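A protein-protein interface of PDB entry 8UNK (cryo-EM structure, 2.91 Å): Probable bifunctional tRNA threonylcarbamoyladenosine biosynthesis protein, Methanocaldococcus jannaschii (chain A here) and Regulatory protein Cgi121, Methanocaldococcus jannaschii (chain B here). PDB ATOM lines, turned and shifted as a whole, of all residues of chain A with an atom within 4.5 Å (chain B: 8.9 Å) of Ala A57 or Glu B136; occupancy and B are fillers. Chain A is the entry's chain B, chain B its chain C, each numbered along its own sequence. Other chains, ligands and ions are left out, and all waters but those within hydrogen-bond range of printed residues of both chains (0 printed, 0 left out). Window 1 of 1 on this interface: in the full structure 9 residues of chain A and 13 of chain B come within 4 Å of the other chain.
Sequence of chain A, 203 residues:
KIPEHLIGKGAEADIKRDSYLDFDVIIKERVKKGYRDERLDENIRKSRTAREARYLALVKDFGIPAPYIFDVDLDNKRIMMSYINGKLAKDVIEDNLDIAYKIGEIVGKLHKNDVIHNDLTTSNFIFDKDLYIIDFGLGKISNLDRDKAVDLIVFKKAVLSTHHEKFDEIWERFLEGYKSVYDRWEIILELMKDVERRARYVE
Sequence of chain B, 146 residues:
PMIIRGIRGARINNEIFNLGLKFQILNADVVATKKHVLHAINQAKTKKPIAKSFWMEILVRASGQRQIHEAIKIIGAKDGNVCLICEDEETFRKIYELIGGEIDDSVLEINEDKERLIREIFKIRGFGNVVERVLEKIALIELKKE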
ATOM      1  N   ALA A  53      -7.928   8.028  35.479  1.00  0.00           N
ATOM      2  CA  ALA A  53      -8.686   7.319  34.456  1.00  0.00           C
ATOM      3  C   ALA A  53      -9.761   8.217  33.863  1.00  0.00           C
ATOM      4  O   ALA A  53      -9.836   8.401  32.639  1.00  0.00           O
ATOM      5  CB  ALA A  53      -9.312   6.056  35.046  1.00  0.00           C
ATOM      6  N   ARG A  54     -10.581   8.818  34.729  1.00  0.00           N
ATOM      7  CA  ARG A  54     -11.710   9.603  34.252  1.00  0.00           C
ATOM      8  C   ARG A  54     -11.252  10.740  33.355  1.00  0.00           C
ATOM      9  O   ARG A  54     -11.833  10.967  32.289  1.00  0.00           O
ATOM     10  CB  ARG A  54     -12.501  10.150  35.436  1.00  0.00           C
ATOM     11  CG  ARG A  54     -13.467  11.256  35.070  1.00  0.00           C
ATOM     12  CD  ARG A  54     -14.729  11.170  35.899  1.00  0.00           C
ATOM     13  NE  ARG A  54     -14.435  11.117  37.327  1.00  0.00           N
ATOM     14  CZ  ARG A  54     -15.128  10.420  38.216  1.00  0.00           C
ATOM     15  NH1 ARG A  54     -16.180   9.697  37.866  1.00  0.00           N
ATOM     16  NH2 ARG A  54     -14.758  10.450  39.493  1.00  0.00           N
ATOM     17  N   TYR A  55     -10.200  11.456  33.752  1.00  0.00           N
ATOM     18  CA  TYR A  55      -9.817  12.640  32.997  1.00  0.00           C
ATOM     19  C   TYR A  55      -8.959  12.308  31.786  1.00  0.00           C
ATOM     20  O   TYR A  55      -9.098  12.968  30.753  1.00  0.00           O
ATOM     21  CB  TYR A  55      -9.111  13.635  33.914  1.00  0.00           C
ATOM     22  CG  TYR A  55     -10.015  14.112  35.023  1.00  0.00           C
ATOM     23  CD1 TYR A  55     -11.274  14.617  34.741  1.00  0.00           C
ATOM     24  CD2 TYR A  55      -9.623  14.043  36.349  1.00  0.00           C
ATOM     25  CE1 TYR A  55     -12.111  15.043  35.741  1.00  0.00           C
ATOM     26  CE2 TYR A  55     -10.457  14.470  37.359  1.00  0.00           C
ATOM     27  CZ  TYR A  55     -11.701  14.971  37.050  1.00  0.00           C
ATOM     28  OH  TYR A  55     -12.538  15.399  38.052  1.00  0.00           O
ATOM     29  N   LEU A  56      -8.091  11.299  31.859  1.00  0.00           N
ATOM     30  CA  LEU A  56      -7.410  10.846  30.656  1.00  0.00           C
ATOM     31  C   LEU A  56      -8.391  10.334  29.618  1.00  0.00           C
ATOM     32  O   LEU A  56      -8.084  10.364  28.423  1.00  0.00           O
ATOM     33  CB  LEU A  56      -6.403   9.746  30.988  1.00  0.00           C
ATOM     34  CG  LEU A  56      -4.958  10.186  31.204  1.00  0.00           C
ATOM     35  CD1 LEU A  56      -4.147   9.055  31.810  1.00  0.00           C
ATOM     36  CD2 LEU A  56      -4.347  10.630  29.889  1.00  0.00           C
ATOM     37  N   ALA A  57      -9.561   9.851  30.041  1.00  0.00           N
ATOM     38  CA  ALA A  57     -10.575   9.479  29.064  1.00  0.00           C
ATOM     39  C   ALA A  57     -11.327  10.702  28.553  1.00  0.00           C
ATOM     40  O   ALA A  57     -11.469  10.890  27.340  1.00  0.00           O
ATOM     41  CB  ALA A  57     -11.546   8.466  29.671  1.00  0.00           C
ATOM     42  N   LEU A  58     -11.806  11.550  29.465  1.00  0.00           N
ATOM     43  CA  LEU A  58     -12.588  12.719  29.079  1.00  0.00           C
ATOM     44  C   LEU A  58     -11.780  13.717  28.263  1.00  0.00           C
ATOM     45  O   LEU A  58     -12.370  14.567  27.589  1.00  0.00           O
ATOM     46  CB  LEU A  58     -13.146  13.392  30.333  1.00  0.00           C
ATOM     47  CG  LEU A  58     -13.723  14.802  30.195  1.00  0.00           C
ATOM     48  CD1 LEU A  58     -14.869  14.992  31.176  1.00  0.00           C
ATOM     49  CD2 LEU A  58     -12.657  15.863  30.423  1.00  0.00           C
ATOM     50  N   VAL A  59     -10.449  13.643  28.311  1.00  0.00           N
ATOM     51  CA  VAL A  59      -9.632  14.614  27.595  1.00  0.00           C
ATOM     52  C   VAL A  59      -9.797  14.454  26.091  1.00  0.00           C
ATOM     53  O   VAL A  59      -9.771  15.443  25.350  1.00  0.00           O
ATOM     54  CB  VAL A  59      -8.158  14.480  28.028  1.00  0.00           C
ATOM     55  CG1 VAL A  59      -7.488  13.311  27.321  1.00  0.00           C
ATOM     56  CG2 VAL A  59      -7.409  15.769  27.781  1.00  0.00           C
ATOM     57  N   LYS A  60      -9.970  13.221  25.610  1.00  0.00           N
ATOM     58  CA  LYS A  60     -10.119  12.991  24.179  1.00  0.00           C
ATOM     59  C   LYS A  60     -11.427  13.539  23.625  1.00  0.00           C
ATOM     60  O   LYS A  60     -11.565  13.639  22.402  1.00  0.00           O
ATOM     61  CB  LYS A  60     -10.021  11.499  23.872  1.00  0.00           C
ATOM     62  CG  LYS A  60      -8.625  11.053  23.488  1.00  0.00           C
ATOM     63  CD  LYS A  60      -8.490   9.543  23.547  1.00  0.00           C
ATOM     64  CE  LYS A  60      -7.057   9.123  23.793  1.00  0.00           C
ATOM     65  NZ  LYS A  60      -6.897   8.504  25.134  1.00  0.00           N
ATOM     66  N   ASP A  61     -12.384  13.894  24.483  1.00  0.00           N
ATOM     67  CA  ASP A  61     -13.591  14.553  24.004  1.00  0.00           C
ATOM     68  C   ASP A  61     -13.287  15.916  23.399  1.00  0.00           C
ATOM     69  O   ASP A  61     -14.141  16.479  22.706  1.00  0.00           O
ATOM     70  CB  ASP A  61     -14.596  14.714  25.146  1.00  0.00           C
ATOM     71  CG  ASP A  61     -15.393  13.452  25.408  1.00  0.00           C
ATOM     72  OD1 ASP A  61     -15.576  12.653  24.467  1.00  0.00           O
ATOM     73  OD2 ASP A  61     -15.839  13.261  26.558  1.00  0.00           O
ATOM     74  N   PRO A  67      -3.113   8.696  25.821  1.00  0.00           N
ATOM     75  CA  PRO A  67      -3.143   7.231  25.790  1.00  0.00           C
ATOM     76  C   PRO A  67      -4.536   6.689  26.073  1.00  0.00           C
ATOM     77  O   PRO A  67      -5.308   7.259  26.847  1.00  0.00           O
ATOM     78  CB  PRO A  67      -2.153   6.823  26.889  1.00  0.00           C
ATOM     79  CG  PRO A  67      -1.404   8.063  27.251  1.00  0.00           C
ATOM     80  CD  PRO A  67      -2.296   9.209  26.931  1.00  0.00           C
ATOM     81  N   TYR A  68      -4.848   5.567  25.429  1.00  0.00           N
ATOM     82  CA  TYR A  68      -6.120   4.892  25.627  1.00  0.00           C
ATOM     83  C   TYR A  68      -6.101   4.084  26.920  1.00  0.00           C
ATOM     84  O   TYR A  68      -5.111   3.436  27.264  1.00  0.00           O
ATOM     85  CB  TYR A  68      -6.424   3.967  24.447  1.00  0.00           C
ATOM     86  CG  TYR A  68      -6.776   4.682  23.162  1.00  0.00           C
ATOM     87  CD1 TYR A  68      -7.769   5.652  23.129  1.00  0.00           C
ATOM     88  CD2 TYR A  68      -6.106   4.393  21.982  1.00  0.00           C
ATOM     89  CE1 TYR A  68      -8.090   6.304  21.957  1.00  0.00           C
ATOM     90  CE2 TYR A  68      -6.417   5.041  20.808  1.00  0.00           C
ATOM     91  CZ  TYR A  68      -7.409   5.996  20.799  1.00  0.00           C
ATOM     92  OH  TYR A  68      -7.721   6.643  19.626  1.00  0.00           O
ATOM     93  N   ILE A  69      -7.226   4.118  27.632  1.00  0.00           N
ATOM     94  CA  ILE A  69      -7.374   3.380  28.883  1.00  0.00           C
ATOM     95  C   ILE A  69      -7.934   2.001  28.564  1.00  0.00           C
ATOM     96  O   ILE A  69      -9.152   1.803  28.537  1.00  0.00           O
ATOM     97  CB  ILE A  69      -8.280   4.139  29.870  1.00  0.00           C
ATOM     98  CG1 ILE A  69      -7.508   5.287  30.516  1.00  0.00           C
ATOM     99  CG2 ILE A  69      -8.807   3.201  30.950  1.00  0.00           C
ATOM    100  CD1 ILE A  69      -8.396   6.305  31.194  1.00  0.00           C
ATOM    101  N   LYS B  35     -13.110  -6.990  19.066  1.00  0.00           N
ATOM    102  CA  LYS B  35     -12.474  -6.367  20.220  1.00  0.00           C
ATOM    103  C   LYS B  35     -13.512  -5.959  21.256  1.00  0.00           C
ATOM    104  O   LYS B  35     -13.265  -6.062  22.460  1.00  0.00           O
ATOM    105  CB  LYS B  35     -11.651  -5.159  19.779  1.00  0.00           C
ATOM    106  N   HIS B  36     -14.677  -5.494  20.807  1.00  0.00           N
ATOM    107  CA  HIS B  36     -15.751  -5.170  21.739  1.00  0.00           C
ATOM    108  C   HIS B  36     -16.148  -6.398  22.549  1.00  0.00           C
ATOM    109  O   HIS B  36     -16.277  -6.336  23.777  1.00  0.00           O
ATOM    110  CB  HIS B  36     -16.950  -4.618  20.970  1.00  0.00           C
ATOM    111  CG  HIS B  36     -17.947  -3.900  21.825  1.00  0.00           C
ATOM    112  ND1 HIS B  36     -18.874  -3.024  21.307  1.00  0.00           N
ATOM    113  CD2 HIS B  36     -18.162  -3.928  23.162  1.00  0.00           C
ATOM    114  CE1 HIS B  36     -19.619  -2.542  22.286  1.00  0.00           C
ATOM    115  NE2 HIS B  36     -19.207  -3.076  23.421  1.00  0.00           N
ATOM    116  N   HIS B  39     -13.281  -7.417  25.000  1.00  0.00           N
ATOM    117  CA  HIS B  39     -13.260  -6.541  26.164  1.00  0.00           C
ATOM    118  C   HIS B  39     -14.431  -6.840  27.088  1.00  0.00           C
ATOM    119  O   HIS B  39     -14.278  -6.852  28.314  1.00  0.00           O
ATOM    120  CB  HIS B  39     -13.281  -5.079  25.725  1.00  0.00           C
ATOM    121  CG  HIS B  39     -12.840  -4.125  26.790  1.00  0.00           C
ATOM    122  ND1 HIS B  39     -13.716  -3.301  27.462  1.00  0.00           N
ATOM    123  CD2 HIS B  39     -11.613  -3.867  27.302  1.00  0.00           C
ATOM    124  CE1 HIS B  39     -13.048  -2.574  28.339  1.00  0.00           C
ATOM    125  NE2 HIS B  39     -11.770  -2.898  28.262  1.00  0.00           N
ATOM    126  N   GLN B  43     -13.886  -8.056  30.938  1.00  0.00           N
ATOM    127  CA  GLN B  43     -14.445  -7.288  32.044  1.00  0.00           C
ATOM    128  C   GLN B  43     -15.428  -8.123  32.852  1.00  0.00           C
ATOM    129  O   GLN B  43     -15.459  -8.038  34.085  1.00  0.00           O
ATOM    130  CB  GLN B  43     -15.121  -6.025  31.515  1.00  0.00           C
ATOM    131  CG  GLN B  43     -14.169  -5.056  30.835  1.00  0.00           C
ATOM    132  CD  GLN B  43     -13.287  -4.318  31.819  1.00  0.00           C
ATOM    133  OE1 GLN B  43     -12.080  -4.546  31.880  1.00  0.00           O
ATOM    134  NE2 GLN B  43     -13.888  -3.426  32.597  1.00  0.00           N
ATOM    135  N   ARG B  61     -21.939  -5.255  29.985  1.00  0.00           N
ATOM    136  CA  ARG B  61     -20.589  -4.741  29.780  1.00  0.00           C
ATOM    137  C   ARG B  61     -20.448  -4.109  28.405  1.00  0.00           C
ATOM    138  O   ARG B  61     -19.852  -3.035  28.263  1.00  0.00           O
ATOM    139  CB  ARG B  61     -19.571  -5.868  29.947  1.00  0.00           C
ATOM    140  CG  ARG B  61     -19.248  -6.213  31.388  1.00  0.00           C
ATOM    141  CD  ARG B  61     -18.391  -5.143  32.036  1.00  0.00           C
ATOM    142  NE  ARG B  61     -17.898  -5.561  33.343  1.00  0.00           N
ATOM    143  CZ  ARG B  61     -17.369  -4.741  34.241  1.00  0.00           C
ATOM    144  NH1 ARG B  61     -17.222  -3.449  33.997  1.00  0.00           N
ATOM    145  NH2 ARG B  61     -16.977  -5.230  35.413  1.00  0.00           N
ATOM    146  N   GLY B  64     -22.072  -0.446  28.102  1.00  0.00           N
ATOM    147  CA  GLY B  64     -21.247   0.643  28.580  1.00  0.00           C
ATOM    148  C   GLY B  64     -21.912   1.600  29.542  1.00  0.00           C
ATOM    149  O   GLY B  64     -21.396   2.706  29.736  1.00  0.00           O
ATOM    150  N   PHE B 122     -23.165   5.550  21.122  1.00  0.00           N
ATOM    151  CA  PHE B 122     -22.338   5.726  22.309  1.00  0.00           C
ATOM    152  C   PHE B 122     -22.086   7.186  22.657  1.00  0.00           C
ATOM    153  O   PHE B 122     -21.440   7.459  23.675  1.00  0.00           O
ATOM    154  CB  PHE B 122     -20.996   5.012  22.127  1.00  0.00           C
ATOM    155  CG  PHE B 122     -21.080   3.523  22.266  1.00  0.00           C
ATOM    156  CD1 PHE B 122     -21.428   2.943  23.474  1.00  0.00           C
ATOM    157  CD2 PHE B 122     -20.815   2.700  21.187  1.00  0.00           C
ATOM    158  CE1 PHE B 122     -21.506   1.571  23.602  1.00  0.00           C
ATOM    159  CE2 PHE B 122     -20.891   1.328  21.308  1.00  0.00           C
ATOM    160  CZ  PHE B 122     -21.238   0.763  22.517  1.00  0.00           C
ATOM    161  N   ILE B 124     -20.059   9.190  21.278  1.00  0.00           N
ATOM    162  CA  ILE B 124     -18.617   9.389  21.207  1.00  0.00           C
ATOM    163  C   ILE B 124     -18.342  10.666  20.426  1.00  0.00           C
ATOM    164  O   ILE B 124     -18.303  10.658  19.190  1.00  0.00           O
ATOM    165  CB  ILE B 124     -17.921   8.175  20.562  1.00  0.00           C
ATOM    166  CG1 ILE B 124     -17.831   7.027  21.567  1.00  0.00           C
ATOM    167  CG2 ILE B 124     -16.534   8.549  20.054  1.00  0.00           C
ATOM    168  CD1 ILE B 124     -17.551   5.681  20.934  1.00  0.00           C
ATOM    169  N   ARG B 125     -18.160  11.773  21.139  1.00  0.00           N
ATOM    170  CA  ARG B 125     -17.899  13.079  20.539  1.00  0.00           C
ATOM    171  C   ARG B 125     -16.476  13.485  20.916  1.00  0.00           C
ATOM    172  O   ARG B 125     -16.253  14.165  21.917  1.00  0.00           O
ATOM    173  CB  ARG B 125     -18.920  14.112  21.008  1.00  0.00           C
ATOM    174  N   GLY B 126     -15.517  13.063  20.102  1.00  0.00           N
ATOM    175  CA  GLY B 126     -14.128  13.367  20.379  1.00  0.00           C
ATOM    176  C   GLY B 126     -13.240  12.845  19.274  1.00  0.00           C
ATOM    177  O   GLY B 126     -13.715  12.401  18.227  1.00  0.00           O
ATOM    178  N   PHE B 127     -11.935  12.901  19.525  1.00  0.00           N
ATOM    179  CA  PHE B 127     -10.925  12.464  18.569  1.00  0.00           C
ATOM    180  C   PHE B 127     -10.289  11.176  19.070  1.00  0.00           C
ATOM    181  O   PHE B 127      -9.748  11.137  20.180  1.00  0.00           O
ATOM    182  CB  PHE B 127      -9.861  13.542  18.366  1.00  0.00           C
ATOM    183  N   GLY B 128     -10.346  10.139  18.251  1.00  0.00           N
ATOM    184  CA  GLY B 128      -9.785   8.850  18.598  1.00  0.00           C
ATOM    185  C   GLY B 128     -10.421   7.748  17.788  1.00  0.00           C
ATOM    186  O   GLY B 128     -11.523   7.881  17.253  1.00  0.00           O
ATOM    187  N   ASN B 129      -9.704   6.631  17.696  1.00  0.00           N
ATOM    188  CA  ASN B 129     -10.213   5.486  16.955  1.00  0.00           C
ATOM    189  C   ASN B 129     -11.500   4.981  17.592  1.00  0.00           C
ATOM    190  O   ASN B 129     -11.653   4.992  18.817  1.00  0.00           O
ATOM    191  CB  ASN B 129      -9.167   4.373  16.917  1.00  0.00           C
ATOM    192  CG  ASN B 129      -8.015   4.691  15.986  1.00  0.00           C
ATOM    193  OD1 ASN B 129      -7.925   5.793  15.446  1.00  0.00           O
ATOM    194  ND2 ASN B 129      -7.126   3.725  15.794  1.00  0.00           N
ATOM    195  N   VAL B 130     -12.436   4.540  16.749  1.00  0.00           N
ATOM    196  CA  VAL B 130     -13.746   4.127  17.249  1.00  0.00           C
ATOM    197  C   VAL B 130     -13.612   2.907  18.151  1.00  0.00           C
ATOM    198  O   VAL B 130     -14.192   2.857  19.242  1.00  0.00           O
ATOM    199  CB  VAL B 130     -14.713   3.860  16.080  1.00  0.00           C
ATOM    200  CG1 VAL B 130     -14.987   5.144  15.317  1.00  0.00           C
ATOM    201  CG2 VAL B 130     -14.171   2.780  15.149  1.00  0.00           C
ATOM    202  N   VAL B 131     -12.842   1.906  17.716  1.00  0.00           N
ATOM    203  CA  VAL B 131     -12.740   0.664  18.478  1.00  0.00           C
ATOM    204  C   VAL B 131     -12.072   0.919  19.825  1.00  0.00           C
ATOM    205  O   VAL B 131     -12.538   0.449  20.871  1.00  0.00           O
ATOM    206  CB  VAL B 131     -11.997  -0.412  17.661  1.00  0.00           C
ATOM    207  CG1 VAL B 131     -12.499  -0.428  16.223  1.00  0.00           C
ATOM    208  CG2 VAL B 131     -10.492  -0.187  17.683  1.00  0.00           C
ATOM    209  N   GLU B 132     -10.978   1.682  19.822  1.00  0.00           N
ATOM    210  CA  GLU B 132     -10.319   2.017  21.078  1.00  0.00           C
ATOM    211  C   GLU B 132     -11.243   2.839  21.961  1.00  0.00           C
ATOM    212  O   GLU B 132     -11.250   2.679  23.185  1.00  0.00           O
ATOM    213  CB  GLU B 132      -9.019   2.775  20.812  1.00  0.00           C
ATOM    214  CG  GLU B 132      -8.096   2.115  19.799  1.00  0.00           C
ATOM    215  CD  GLU B 132      -7.461   0.846  20.326  1.00  0.00           C
ATOM    216  OE1 GLU B 132      -8.191  -0.013  20.861  1.00  0.00           O
ATOM    217  OE2 GLU B 132      -6.227   0.706  20.200  1.00  0.00           O
ATOM    218  N   ARG B 133     -12.036   3.720  21.355  1.00  0.00           N
ATOM    219  CA  ARG B 133     -12.934   4.551  22.146  1.00  0.00           C
ATOM    220  C   ARG B 133     -14.023   3.718  22.809  1.00  0.00           C
ATOM    221  O   ARG B 133     -14.394   3.985  23.954  1.00  0.00           O
ATOM    222  CB  ARG B 133     -13.546   5.648  21.277  1.00  0.00           C
ATOM    223  CG  ARG B 133     -13.966   6.871  22.071  1.00  0.00           C
ATOM    224  CD  ARG B 133     -12.882   7.938  22.059  1.00  0.00           C
ATOM    225  NE  ARG B 133     -12.974   8.811  23.222  1.00  0.00           N
ATOM    226  CZ  ARG B 133     -13.684   9.929  23.272  1.00  0.00           C
ATOM    227  NH1 ARG B 133     -14.373  10.361  22.228  1.00  0.00           N
ATOM    228  NH2 ARG B 133     -13.708  10.632  24.399  1.00  0.00           N
ATOM    229  N   VAL B 134     -14.553   2.705  22.116  1.00  0.00           N
ATOM    230  CA  VAL B 134     -15.573   1.869  22.748  1.00  0.00           C
ATOM    231  C   VAL B 134     -14.944   1.003  23.833  1.00  0.00           C
ATOM    232  O   VAL B 134     -15.539   0.789  24.898  1.00  0.00           O
ATOM    233  CB  VAL B 134     -16.332   1.004  21.720  1.00  0.00           C
ATOM    234  CG1 VAL B 134     -17.433   1.814  21.043  1.00  0.00           C
ATOM    235  CG2 VAL B 134     -15.399   0.346  20.719  1.00  0.00           C
ATOM    236  N   LEU B 135     -13.742   0.475  23.582  1.00  0.00           N
ATOM    237  CA  LEU B 135     -13.029  -0.251  24.629  1.00  0.00           C
ATOM    238  C   LEU B 135     -12.887   0.616  25.873  1.00  0.00           C
ATOM    239  O   LEU B 135     -13.165   0.179  26.995  1.00  0.00           O
ATOM    240  CB  LEU B 135     -11.651  -0.680  24.123  1.00  0.00           C
ATOM    241  CG  LEU B 135     -11.522  -2.064  23.486  1.00  0.00           C
ATOM    242  CD1 LEU B 135     -12.727  -2.386  22.621  1.00  0.00           C
ATOM    243  CD2 LEU B 135     -10.239  -2.146  22.673  1.00  0.00           C
ATOM    244  N   GLU B 136     -12.455   1.862  25.678  1.00  0.00           N
ATOM    245  CA  GLU B 136     -12.285   2.794  26.785  1.00  0.00           C
ATOM    246  C   GLU B 136     -13.613   3.095  27.469  1.00  0.00           C
ATOM    247  O   GLU B 136     -13.677   3.204  28.698  1.00  0.00           O
ATOM    248  CB  GLU B 136     -11.640   4.071  26.253  1.00  0.00           C
ATOM    249  CG  GLU B 136     -11.192   5.058  27.296  1.00  0.00           C
ATOM    250  CD  GLU B 136     -10.247   6.093  26.723  1.00  0.00           C
ATOM    251  OE1 GLU B 136     -10.418   7.286  27.030  1.00  0.00           O
ATOM    252  OE2 GLU B 136      -9.329   5.712  25.966  1.00  0.00           O
ATOM    253  N   LYS B 137     -14.682   3.246  26.686  1.00  0.00           N
ATOM    254  CA  LYS B 137     -15.993   3.528  27.257  1.00  0.00           C
ATOM    255  C   LYS B 137     -16.457   2.383  28.145  1.00  0.00           C
ATOM    256  O   LYS B 137     -17.024   2.608  29.220  1.00  0.00           O
ATOM    257  CB  LYS B 137     -16.998   3.781  26.132  1.00  0.00           C
ATOM    258  CG  LYS B 137     -18.410   4.117  26.593  1.00  0.00           C
ATOM    259  CD  LYS B 137     -18.474   5.470  27.277  1.00  0.00           C
ATOM    260  CE  LYS B 137     -19.168   5.373  28.623  1.00  0.00           C
ATOM    261  NZ  LYS B 137     -18.388   4.558  29.595  1.00  0.00           N
ATOM    262  N   ILE B 138     -16.232   1.144  27.705  1.00  0.00           N
ATOM    263  CA  ILE B 138     -16.615  -0.009  28.513  1.00  0.00           C
ATOM    264  C   ILE B 138     -15.748  -0.097  29.762  1.00  0.00           C
ATOM    265  O   ILE B 138     -16.245  -0.378  30.859  1.00  0.00           O
ATOM    266  CB  ILE B 138     -16.536  -1.300  27.676  1.00  0.00           C
ATOM    267  CG1 ILE B 138     -17.489  -1.239  26.474  1.00  0.00           C
ATOM    268  CG2 ILE B 138     -16.852  -2.509  28.539  1.00  0.00           C
ATOM    269  CD1 ILE B 138     -18.813  -0.548  26.739  1.00  0.00           C
ATOM    270  N   ALA B 139     -14.442   0.143  29.621  1.00  0.00           N
ATOM    271  CA  ALA B 139     -13.558   0.091  30.780  1.00  0.00           C
ATOM    272  C   ALA B 139     -13.959   1.126  31.823  1.00  0.00           C
ATOM    273  O   ALA B 139     -13.945   0.844  33.026  1.00  0.00           O
ATOM    274  CB  ALA B 139     -12.108   0.303  30.348  1.00  0.00           C
ATOM    275  N   LEU B 140     -14.328   2.325  31.381  1.00  0.00           N
ATOM    276  CA  LEU B 140     -14.733   3.389  32.291  1.00  0.00           C
ATOM    277  C   LEU B 140     -16.059   3.109  32.985  1.00  0.00           C
ATOM    278  O   LEU B 140     -16.516   3.958  33.759  1.00  0.00           O
ATOM    279  CB  LEU B 140     -14.823   4.714  31.530  1.00  0.00           C
ATOM    280  CG  LEU B 140     -13.593   5.623  31.596  1.00  0.00           C
ATOM    281  CD1 LEU B 140     -13.536   6.332  32.937  1.00  0.00           C
ATOM    282  CD2 LEU B 140     -12.311   4.844  31.344  1.00  0.00           C
ATOM    283  N   ILE B 141     -16.688   1.958  32.735  1.00  0.00           N
ATOM    284  CA  ILE B 141     -17.934   1.636  33.423  1.00  0.00           C
ATOM    285  C   ILE B 141     -17.718   1.583  34.926  1.00  0.00           C
ATOM    286  O   ILE B 141     -18.648   1.824  35.706  1.00  0.00           O
ATOM    287  CB  ILE B 141     -18.508   0.309  32.891  1.00  0.00           C
ATOM    288  N   GLU B 142     -16.497   1.271  35.361  1.00  0.00           N
ATOM    289  CA  GLU B 142     -16.158   1.214  36.784  1.00  0.00           C
ATOM    290  C   GLU B 142     -15.851   2.629  37.266  1.00  0.00           C
ATOM    291  O   GLU B 142     -14.699   3.061  37.358  1.00  0.00           O
ATOM    292  CB  GLU B 142     -14.982   0.277  37.019  1.00  0.00           C
ATOM    293  CG  GLU B 142     -15.231  -1.157  36.579  1.00  0.00           C
ATOM    294  CD  GLU B 142     -13.979  -1.829  36.055  1.00  0.00           C
ATOM    295  OE1 GLU B 142     -13.247  -1.192  35.269  1.00  0.00           O
ATOM    296  OE2 GLU B 142     -13.726  -2.992  36.431  1.00  0.00           O
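Of the 12 printed residues of chain A, 6 touch a printed residue of chain B. Printed residues of chain A that touch a printed residue of chain B: Arg A54, Ala A57, Lys A60, Asp A61, Tyr A68 and Ile A69. Hydrophobic or aromatic side chains of chain A within 4 Å of the printed part of chain B: Ala A57, Tyr A68 and Ile A69. Of the 26 printed residues of chain B, 10 touch a printed residue of chain A.
The side-chain amino group (NZ) of Lys A60 is in hydrogen-bond range of the backbone carbonyl oxygen (O) of Pro A67, 2.6 Å away.
Leu A56 touches none of the printed residues of chain B. Of the printed residues of chain B, Ala A57 touches Arg B133, Glu B136 and Leu B140. Of the printed residues of chain B, Ile A69 touches Glu B136 (3.1 Å), Ala B139 (3.8 Å) and Leu B140 (3.9 Å). Printed residues of chain A within 4 Å of Arg B133: Ala A57, Lys A60 and Asp A61. Of chain A, only Ala A57, Lys A60, Tyr A68 and Ile A69 come within 4 Å of Glu B136. Ile B138 touches none of the printed residues of chain A. Of the printed residues of chain A, Ala B139 touches Ile A69. The nearest printed residue of chain B that does not touch Ala A57 is Lys B137 (6.8 Å). The nearest residue of chain A that does not touch Glu B136 is Leu A56 (4.1 Å). The nearest printed residue of chain A that does not touch Arg B133 is Tyr A68 (4.8 Å).
O of Lys A60 lies within hydrogen-bond range of N of Phe B127 (3.0 Å). The side-chain carboxylate of Glu B136 lies within salt-bridge range of the side-chain amino group of Lys A60 (3.8 Å). The side-chain carboxylate (OD1) of Asp A61 lies within salt-bridge range of the guanidinium group (NH2) of Arg B133, at 2.8 Å. The backbone NH (N) of Asn B129 is in hydrogen-bond range of the side-chain hydroxyl (OH) of Tyr A68 (2.8 Å). The backbone NH (N) of Ile A69 sits at hydrogen-bond distance from the side-chain carboxylate (OE2) of Glu B136 (3.1 Å). The side-chain carboxylate (OD1) of Asp A61 lies close to the backbone carbonyl oxygen (O) of Arg B125, at 3.0 Å.
Among the printed residues, merely in contact across the chains: Ala A57 with Glu B136 (3.0 Å), Tyr A68 with Gly B128 (3.2 Å), Tyr A68 with Glu B136 (3.2 Å), Lys A60 with Gly B126 (3.3 Å), Tyr A68 with Glu B132 (3.5 Å), Ala A57 with Arg B133 (3.7 Å), Lys A60 with Arg B133 (3.8 Å), Ile A69 with Ala B139 (3.8 Å), Asp A61 with Gly B126 (3.9 Å), Ile A69 with Leu B140 (3.9 Å), Arg A54 with Leu B140 (3.97 Å) and Ala A57 with Leu B140 (3.997 Å).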
